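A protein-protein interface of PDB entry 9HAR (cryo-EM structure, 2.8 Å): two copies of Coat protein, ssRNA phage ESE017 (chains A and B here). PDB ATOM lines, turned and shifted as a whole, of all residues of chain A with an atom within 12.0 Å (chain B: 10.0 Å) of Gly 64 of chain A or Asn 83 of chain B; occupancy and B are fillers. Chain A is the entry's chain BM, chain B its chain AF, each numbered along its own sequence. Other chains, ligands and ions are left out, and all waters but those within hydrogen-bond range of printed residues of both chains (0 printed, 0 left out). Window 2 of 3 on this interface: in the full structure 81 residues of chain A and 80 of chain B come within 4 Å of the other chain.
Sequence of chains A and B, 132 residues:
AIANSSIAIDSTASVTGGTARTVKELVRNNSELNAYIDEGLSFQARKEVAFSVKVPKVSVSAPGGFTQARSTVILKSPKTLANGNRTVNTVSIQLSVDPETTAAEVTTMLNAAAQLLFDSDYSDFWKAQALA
No position is printed for both chains. Of the 10 pairs that touch across the chains among the printed residues, none has its exchanged pair printed and touching as well.
ND2 of Asn 83 of chain B sits close to N of Asn 85 of chain B, at 3.0 Å. OD1 of Asp 98 of chain A is in hydrogen-bond range of N of Glu 100 of chain A. The backbone NH of Lys 79 of chain B sits at hydrogen-bond distance from the backbone carbonyl oxygen of Thr 87 of chain B (2.9 Å).
No residue of chain B comes within 4 Å of Ala 62 of chain A. Pro 63 of chain A touches just these residues of chain B: Leu 81 and Asn 85. Of the printed residues of chain B, Gly 64 of chain A touches Leu 81 (3.5 Å) and Asn 83 (3.2 Å). No residue of chain B comes within 4 Å of Gly 65 of chain A. No residue of chain B comes within 4 Å of Phe 66 of chain A. Val 97 of chain A touches none of the printed residues of chain B. Of the printed residues of chain B, Asp 98 of chain A touches Leu 81 and Thr 87. Ala 82 of chain B touches just one residue of chain A: Glu 100 (3.1 Å). Of the printed residues of chain A, Asn 83 of chain B touches Gly 64 and Glu 100. No residue of chain A comes within 4 Å of Gly 84 of chain B. Asn 85 of chain B touches just one residue of chain A: Pro 63. Of the printed residues of chain A, Val 88 of chain B touches Gln 68. The nearest residue of chain B that does not touch Gly 64 of chain A is Asn 85 of chain B (5.0 Å). The nearest printed residue of chain A that does not touch Val 88 of chain B is Asp 98 of chain A (5.1 Å).
Hydrophobic or aromatic side chains of chain A within 4 Å of the printed part of chain B: Pro 63. Printed residues of chain B that touch a printed residue of chain A: Lys 79, Leu 81, Ala 82, Asn 83, Asn 85, Thr 87 and Val 88. Hydrophobic or aromatic side chains of chain B within 4 Å of the printed part of chain A: Leu 81 and Ala 82. Among the printed residues, 10 pairs touch across the chains. Among the printed residues, no Asp or Glu carboxylate lies within 4 Å of a Lys or Arg side-chain nitrogen of the other chain.
Among the printed residues, merely in contact across the chains: Pro 63 of chain A with Leu 81 of chain B, Pro 63 of chain A with Asn 85 of chain B, Gly 64 of chain A with Leu 81 of chain B, Gly 64 of chain A with Asn 83 of chain B, Asp 98 of chain A with Leu 81 of chain B, Asp 98 of chain A with Thr 87 of chain B, Glu 100 of chain A with Asn 83 of chain B and Thr 101 of chain A with Lys 79 of chain B.
OE1 of Gln 68 of chain A sits close to O of Val 88 of chain B, 3.1 Å away. The side-chain carboxylate (OE1) of Glu 100 of chain A lies within hydrogen-bond range of the backbone NH (N) of Ala 82 of chain B (3.1 Å).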
ATOM      1  N   PRO A  56      13.561 -23.948 -26.024  1.00  0.00           N
ATOM      2  CA  PRO A  56      14.325 -22.771 -26.455  1.00  0.00           C
ATOM      3  C   PRO A  56      13.499 -21.816 -27.306  1.00  0.00           C
ATOM      4  O   PRO A  56      12.527 -22.187 -27.969  1.00  0.00           O
ATOM      5  CB  PRO A  56      15.478 -23.373 -27.265  1.00  0.00           C
ATOM      6  CG  PRO A  56      15.528 -24.805 -26.867  1.00  0.00           C
ATOM      7  CD  PRO A  56      14.123 -25.190 -26.577  1.00  0.00           C
ATOM      8  N   LYS A  57      13.921 -20.554 -27.288  1.00  0.00           N
ATOM      9  CA  LYS A  57      13.267 -19.488 -28.038  1.00  0.00           C
ATOM     10  C   LYS A  57      14.337 -18.710 -28.787  1.00  0.00           C
ATOM     11  O   LYS A  57      15.320 -18.274 -28.179  1.00  0.00           O
ATOM     12  CB  LYS A  57      12.482 -18.563 -27.105  1.00  0.00           C
ATOM     13  CG  LYS A  57      11.368 -17.790 -27.776  1.00  0.00           C
ATOM     14  CD  LYS A  57      10.731 -16.806 -26.810  1.00  0.00           C
ATOM     15  CE  LYS A  57       9.845 -15.809 -27.541  1.00  0.00           C
ATOM     16  NZ  LYS A  57       8.418 -16.226 -27.529  1.00  0.00           N
ATOM     17  N   VAL A  58      14.139 -18.520 -30.092  1.00  0.00           N
ATOM     18  CA  VAL A  58      15.163 -17.939 -30.957  1.00  0.00           C
ATOM     19  C   VAL A  58      15.471 -16.511 -30.527  1.00  0.00           C
ATOM     20  O   VAL A  58      14.615 -15.622 -30.617  1.00  0.00           O
ATOM     21  CB  VAL A  58      14.739 -17.987 -32.436  1.00  0.00           C
ATOM     22  CG1 VAL A  58      15.673 -17.133 -33.281  1.00  0.00           C
ATOM     23  CG2 VAL A  58      14.730 -19.419 -32.938  1.00  0.00           C
ATOM     24  N   SER A  59      16.692 -16.284 -30.059  1.00  0.00           N
ATOM     25  CA  SER A  59      17.133 -14.984 -29.589  1.00  0.00           C
ATOM     26  C   SER A  59      18.208 -14.418 -30.524  1.00  0.00           C
ATOM     27  O   SER A  59      18.620 -15.072 -31.490  1.00  0.00           O
ATOM     28  CB  SER A  59      17.629 -15.118 -28.146  1.00  0.00           C
ATOM     29  OG  SER A  59      18.983 -15.531 -28.122  1.00  0.00           O
ATOM     30  N   VAL A  60      18.666 -13.200 -30.240  1.00  0.00           N
ATOM     31  CA  VAL A  60      19.799 -12.596 -30.925  1.00  0.00           C
ATOM     32  C   VAL A  60      21.066 -12.688 -30.084  1.00  0.00           C
ATOM     33  O   VAL A  60      22.167 -12.842 -30.618  1.00  0.00           O
ATOM     34  CB  VAL A  60      19.480 -11.128 -31.293  1.00  0.00           C
ATOM     35  CG1 VAL A  60      18.704 -10.458 -30.168  1.00  0.00           C
ATOM     36  CG2 VAL A  60      20.747 -10.346 -31.614  1.00  0.00           C
ATOM     37  N   SER A  61      20.914 -12.646 -28.768  1.00  0.00           N
ATOM     38  CA  SER A  61      21.933 -12.924 -27.773  1.00  0.00           C
ATOM     39  C   SER A  61      22.104 -14.443 -27.689  1.00  0.00           C
ATOM     40  O   SER A  61      21.806 -15.160 -28.653  1.00  0.00           O
ATOM     41  CB  SER A  61      21.540 -12.283 -26.438  1.00  0.00           C
ATOM     42  OG  SER A  61      20.865 -11.056 -26.642  1.00  0.00           O
ATOM     43  N   ALA A  62      22.632 -14.940 -26.560  1.00  0.00           N
ATOM     44  CA  ALA A  62      22.818 -16.377 -26.368  1.00  0.00           C
ATOM     45  C   ALA A  62      23.854 -16.926 -27.340  1.00  0.00           C
ATOM     46  O   ALA A  62      23.506 -17.473 -28.395  1.00  0.00           O
ATOM     47  CB  ALA A  62      21.494 -17.133 -26.502  1.00  0.00           C
ATOM     48  N   PRO A  63      25.139 -16.784 -27.013  1.00  0.00           N
ATOM     49  CA  PRO A  63      26.208 -17.060 -27.982  1.00  0.00           C
ATOM     50  C   PRO A  63      26.256 -18.524 -28.380  1.00  0.00           C
ATOM     51  O   PRO A  63      26.949 -19.344 -27.770  1.00  0.00           O
ATOM     52  CB  PRO A  63      27.483 -16.630 -27.241  1.00  0.00           C
ATOM     53  CG  PRO A  63      27.041 -16.177 -25.853  1.00  0.00           C
ATOM     54  CD  PRO A  63      25.656 -16.676 -25.642  1.00  0.00           C
ATOM     55  N   GLY A  64      25.498 -18.841 -29.425  1.00  0.00           N
ATOM     56  CA  GLY A  64      25.126 -20.191 -29.791  1.00  0.00           C
ATOM     57  C   GLY A  64      23.776 -20.162 -30.474  1.00  0.00           C
ATOM     58  O   GLY A  64      23.314 -21.165 -31.025  1.00  0.00           O
ATOM     59  N   GLY A  65      23.140 -18.993 -30.445  1.00  0.00           N
ATOM     60  CA  GLY A  65      21.961 -18.737 -31.247  1.00  0.00           C
ATOM     61  C   GLY A  65      20.712 -18.392 -30.467  1.00  0.00           C
ATOM     62  O   GLY A  65      20.009 -17.441 -30.822  1.00  0.00           O
ATOM     63  N   PHE A  66      20.427 -19.135 -29.401  1.00  0.00           N
ATOM     64  CA  PHE A  66      19.207 -18.949 -28.628  1.00  0.00           C
ATOM     65  C   PHE A  66      19.255 -19.730 -27.317  1.00  0.00           C
ATOM     66  O   PHE A  66      20.122 -20.578 -27.093  1.00  0.00           O
ATOM     67  CB  PHE A  66      17.990 -19.308 -29.484  1.00  0.00           C
ATOM     68  CG  PHE A  66      18.115 -20.610 -30.209  1.00  0.00           C
ATOM     69  CD1 PHE A  66      18.037 -21.819 -29.547  1.00  0.00           C
ATOM     70  CD2 PHE A  66      18.358 -20.613 -31.568  1.00  0.00           C
ATOM     71  CE1 PHE A  66      18.159 -23.001 -30.243  1.00  0.00           C
ATOM     72  CE2 PHE A  66      18.494 -21.788 -32.255  1.00  0.00           C
ATOM     73  CZ  PHE A  66      18.391 -22.986 -31.596  1.00  0.00           C
ATOM     74  N   THR A  67      18.297 -19.414 -26.448  1.00  0.00           N
ATOM     75  CA  THR A  67      18.316 -19.820 -25.051  1.00  0.00           C
ATOM     76  C   THR A  67      18.305 -21.338 -24.906  1.00  0.00           C
ATOM     77  O   THR A  67      17.977 -22.083 -25.831  1.00  0.00           O
ATOM     78  CB  THR A  67      17.118 -19.235 -24.307  1.00  0.00           C
ATOM     79  OG1 THR A  67      15.967 -20.052 -24.548  1.00  0.00           O
ATOM     80  CG2 THR A  67      16.829 -17.825 -24.789  1.00  0.00           C
ATOM     81  N   GLN A  68      18.663 -21.787 -23.709  1.00  0.00           N
ATOM     82  CA  GLN A  68      18.733 -23.206 -23.411  1.00  0.00           C
ATOM     83  C   GLN A  68      17.340 -23.778 -23.158  1.00  0.00           C
ATOM     84  O   GLN A  68      16.376 -23.058 -22.889  1.00  0.00           O
ATOM     85  CB  GLN A  68      19.640 -23.449 -22.210  1.00  0.00           C
ATOM     86  CG  GLN A  68      20.972 -22.737 -22.294  1.00  0.00           C
ATOM     87  CD  GLN A  68      21.687 -22.692 -20.964  1.00  0.00           C
ATOM     88  OE1 GLN A  68      22.493 -23.568 -20.650  1.00  0.00           O
ATOM     89  NE2 GLN A  68      21.396 -21.669 -20.171  1.00  0.00           N
ATOM     90  N   ALA A  69      17.248 -25.100 -23.255  1.00  0.00           N
ATOM     91  CA  ALA A  69      16.008 -25.825 -23.010  1.00  0.00           C
ATOM     92  C   ALA A  69      15.999 -26.293 -21.560  1.00  0.00           C
ATOM     93  O   ALA A  69      16.831 -27.115 -21.165  1.00  0.00           O
ATOM     94  CB  ALA A  69      15.884 -27.009 -23.964  1.00  0.00           C
ATOM     95  N   VAL A  97      20.334 -26.717 -20.153  1.00  0.00           N
ATOM     96  CA  VAL A  97      21.346 -27.160 -21.105  1.00  0.00           C
ATOM     97  C   VAL A  97      21.086 -26.528 -22.465  1.00  0.00           C
ATOM     98  O   VAL A  97      19.941 -26.361 -22.895  1.00  0.00           O
ATOM     99  CB  VAL A  97      21.416 -28.699 -21.231  1.00  0.00           C
ATOM    100  CG1 VAL A  97      21.340 -29.335 -19.874  1.00  0.00           C
ATOM    101  CG2 VAL A  97      20.313 -29.227 -22.118  1.00  0.00           C
ATOM    102  N   ASP A  98      22.173 -26.174 -23.142  1.00  0.00           N
ATOM    103  CA  ASP A  98      22.067 -25.540 -24.446  1.00  0.00           C
ATOM    104  C   ASP A  98      21.459 -26.521 -25.447  1.00  0.00           C
ATOM    105  O   ASP A  98      21.837 -27.699 -25.472  1.00  0.00           O
ATOM    106  CB  ASP A  98      23.443 -25.065 -24.917  1.00  0.00           C
ATOM    107  CG  ASP A  98      23.424 -24.507 -26.324  1.00  0.00           C
ATOM    108  OD1 ASP A  98      23.475 -25.304 -27.281  1.00  0.00           O
ATOM    109  OD2 ASP A  98      23.354 -23.269 -26.473  1.00  0.00           O
ATOM    110  N   PRO A  99      20.520 -26.070 -26.284  1.00  0.00           N
ATOM    111  CA  PRO A  99      19.773 -27.001 -27.146  1.00  0.00           C
ATOM    112  C   PRO A  99      20.624 -27.756 -28.149  1.00  0.00           C
ATOM    113  O   PRO A  99      20.175 -28.796 -28.648  1.00  0.00           O
ATOM    114  CB  PRO A  99      18.771 -26.084 -27.854  1.00  0.00           C
ATOM    115  CG  PRO A  99      19.397 -24.749 -27.795  1.00  0.00           C
ATOM    116  CD  PRO A  99      20.094 -24.678 -26.486  1.00  0.00           C
ATOM    117  N   GLU A 100      21.823 -27.279 -28.463  1.00  0.00           N
ATOM    118  CA  GLU A 100      22.713 -27.978 -29.376  1.00  0.00           C
ATOM    119  C   GLU A 100      23.355 -29.210 -28.754  1.00  0.00           C
ATOM    120  O   GLU A 100      24.011 -29.972 -29.472  1.00  0.00           O
ATOM    121  CB  GLU A 100      23.810 -27.031 -29.865  1.00  0.00           C
ATOM    122  CG  GLU A 100      24.155 -27.175 -31.328  1.00  0.00           C
ATOM    123  CD  GLU A 100      25.052 -26.058 -31.819  1.00  0.00           C
ATOM    124  OE1 GLU A 100      26.134 -26.360 -32.362  1.00  0.00           O
ATOM    125  OE2 GLU A 100      24.672 -24.878 -31.663  1.00  0.00           O
ATOM    126  N   THR A 101      23.190 -29.420 -27.451  1.00  0.00           N
ATOM    127  CA  THR A 101      23.877 -30.516 -26.784  1.00  0.00           C
ATOM    128  C   THR A 101      23.288 -31.859 -27.197  1.00  0.00           C
ATOM    129  O   THR A 101      22.093 -31.979 -27.479  1.00  0.00           O
ATOM    130  CB  THR A 101      23.819 -30.338 -25.261  1.00  0.00           C
ATOM    131  OG1 THR A 101      24.827 -31.145 -24.646  1.00  0.00           O
ATOM    132  CG2 THR A 101      22.470 -30.734 -24.704  1.00  0.00           C
ATOM    133  N   LYS B  79      30.706 -26.783 -22.645  1.00  0.00           N
ATOM    134  CA  LYS B  79      30.520 -27.347 -23.971  1.00  0.00           C
ATOM    135  C   LYS B  79      30.869 -26.305 -25.022  1.00  0.00           C
ATOM    136  O   LYS B  79      30.421 -25.157 -24.943  1.00  0.00           O
ATOM    137  CB  LYS B  79      29.077 -27.827 -24.162  1.00  0.00           C
ATOM    138  CG  LYS B  79      28.678 -28.031 -25.602  1.00  0.00           C
ATOM    139  CD  LYS B  79      27.773 -29.228 -25.747  1.00  0.00           C
ATOM    140  CE  LYS B  79      27.287 -29.367 -27.174  1.00  0.00           C
ATOM    141  NZ  LYS B  79      27.835 -30.593 -27.808  1.00  0.00           N
ATOM    142  N   THR B  80      31.664 -26.714 -26.011  1.00  0.00           N
ATOM    143  CA  THR B  80      32.014 -25.862 -27.142  1.00  0.00           C
ATOM    144  C   THR B  80      31.029 -26.138 -28.272  1.00  0.00           C
ATOM    145  O   THR B  80      30.896 -27.278 -28.728  1.00  0.00           O
ATOM    146  CB  THR B  80      33.450 -26.104 -27.603  1.00  0.00           C
ATOM    147  OG1 THR B  80      34.336 -26.057 -26.479  1.00  0.00           O
ATOM    148  CG2 THR B  80      33.863 -25.038 -28.606  1.00  0.00           C
ATOM    149  N   LEU B  81      30.340 -25.092 -28.721  1.00  0.00           N
ATOM    150  CA  LEU B  81      29.330 -25.249 -29.756  1.00  0.00           C
ATOM    151  C   LEU B  81      29.965 -25.272 -31.142  1.00  0.00           C
ATOM    152  O   LEU B  81      31.153 -24.987 -31.315  1.00  0.00           O
ATOM    153  CB  LEU B  81      28.299 -24.128 -29.656  1.00  0.00           C
ATOM    154  CG  LEU B  81      27.624 -24.043 -28.288  1.00  0.00           C
ATOM    155  CD1 LEU B  81      26.434 -23.116 -28.327  1.00  0.00           C
ATOM    156  CD2 LEU B  81      27.194 -25.428 -27.838  1.00  0.00           C
ATOM    157  N   ALA B  82      29.155 -25.643 -32.138  1.00  0.00           N
ATOM    158  CA  ALA B  82      29.647 -25.709 -33.511  1.00  0.00           C
ATOM    159  C   ALA B  82      30.040 -24.330 -34.024  1.00  0.00           C
ATOM    160  O   ALA B  82      31.029 -24.191 -34.754  1.00  0.00           O
ATOM    161  CB  ALA B  82      28.592 -26.339 -34.418  1.00  0.00           C
ATOM    162  N   ASN B  83      29.276 -23.298 -33.658  1.00  0.00           N
ATOM    163  CA  ASN B  83      29.620 -21.941 -34.072  1.00  0.00           C
ATOM    164  C   ASN B  83      30.975 -21.510 -33.524  1.00  0.00           C
ATOM    165  O   ASN B  83      31.581 -20.568 -34.044  1.00  0.00           O
ATOM    166  CB  ASN B  83      28.529 -20.966 -33.634  1.00  0.00           C
ATOM    167  CG  ASN B  83      28.116 -21.163 -32.191  1.00  0.00           C
ATOM    168  OD1 ASN B  83      27.036 -21.683 -31.909  1.00  0.00           O
ATOM    169  ND2 ASN B  83      28.971 -20.748 -31.269  1.00  0.00           N
ATOM    170  N   GLY B  84      31.460 -22.174 -32.480  1.00  0.00           N
ATOM    171  CA  GLY B  84      32.796 -21.910 -31.990  1.00  0.00           C
ATOM    172  C   GLY B  84      32.829 -21.392 -30.569  1.00  0.00           C
ATOM    173  O   GLY B  84      33.816 -21.593 -29.856  1.00  0.00           O
ATOM    174  N   ASN B  85      31.758 -20.727 -30.146  1.00  0.00           N
ATOM    175  CA  ASN B  85      31.698 -20.166 -28.806  1.00  0.00           C
ATOM    176  C   ASN B  85      31.529 -21.275 -27.769  1.00  0.00           C
ATOM    177  O   ASN B  85      31.392 -22.458 -28.091  1.00  0.00           O
ATOM    178  CB  ASN B  85      30.572 -19.141 -28.702  1.00  0.00           C
ATOM    179  CG  ASN B  85      30.408 -18.325 -29.964  1.00  0.00           C
ATOM    180  OD1 ASN B  85      30.196 -18.870 -31.045  1.00  0.00           O
ATOM    181  ND2 ASN B  85      30.497 -17.007 -29.832  1.00  0.00           N
ATOM    182  N   ARG B  86      31.537 -20.878 -26.503  1.00  0.00           N
ATOM    183  CA  ARG B  86      31.471 -21.787 -25.370  1.00  0.00           C
ATOM    184  C   ARG B  86      30.235 -21.470 -24.540  1.00  0.00           C
ATOM    185  O   ARG B  86      29.804 -20.320 -24.437  1.00  0.00           O
ATOM    186  CB  ARG B  86      32.738 -21.678 -24.513  1.00  0.00           C
ATOM    187  CG  ARG B  86      32.851 -22.711 -23.412  1.00  0.00           C
ATOM    188  CD  ARG B  86      33.229 -22.062 -22.096  1.00  0.00           C
ATOM    189  NE  ARG B  86      33.737 -23.027 -21.129  1.00  0.00           N
ATOM    190  CZ  ARG B  86      34.034 -22.738 -19.870  1.00  0.00           C
ATOM    191  NH1 ARG B  86      33.883 -21.517 -19.388  1.00  0.00           N
ATOM    192  NH2 ARG B  86      34.496 -23.698 -19.075  1.00  0.00           N
ATOM    193  N   THR B  87      29.661 -22.507 -23.947  1.00  0.00           N
ATOM    194  CA  THR B  87      28.489 -22.363 -23.090  1.00  0.00           C
ATOM    195  C   THR B  87      28.624 -23.390 -21.971  1.00  0.00           C
ATOM    196  O   THR B  87      29.503 -24.258 -22.013  1.00  0.00           O
ATOM    197  CB  THR B  87      27.195 -22.532 -23.889  1.00  0.00           C
ATOM    198  OG1 THR B  87      26.091 -22.014 -23.136  1.00  0.00           O
ATOM    199  CG2 THR B  87      26.948 -24.004 -24.204  1.00  0.00           C
ATOM    200  N   VAL B  88      27.775 -23.281 -20.955  1.00  0.00           N
ATOM    201  CA  VAL B  88      27.771 -24.227 -19.844  1.00  0.00           C
ATOM    202  C   VAL B  88      26.381 -24.829 -19.721  1.00  0.00           C
ATOM    203  O   VAL B  88      25.378 -24.108 -19.736  1.00  0.00           O
ATOM    204  CB  VAL B  88      28.190 -23.568 -18.514  1.00  0.00           C
ATOM    205  CG1 VAL B  88      28.600 -24.633 -17.514  1.00  0.00           C
ATOM    206  CG2 VAL B  88      29.319 -22.583 -18.732  1.00  0.00           C
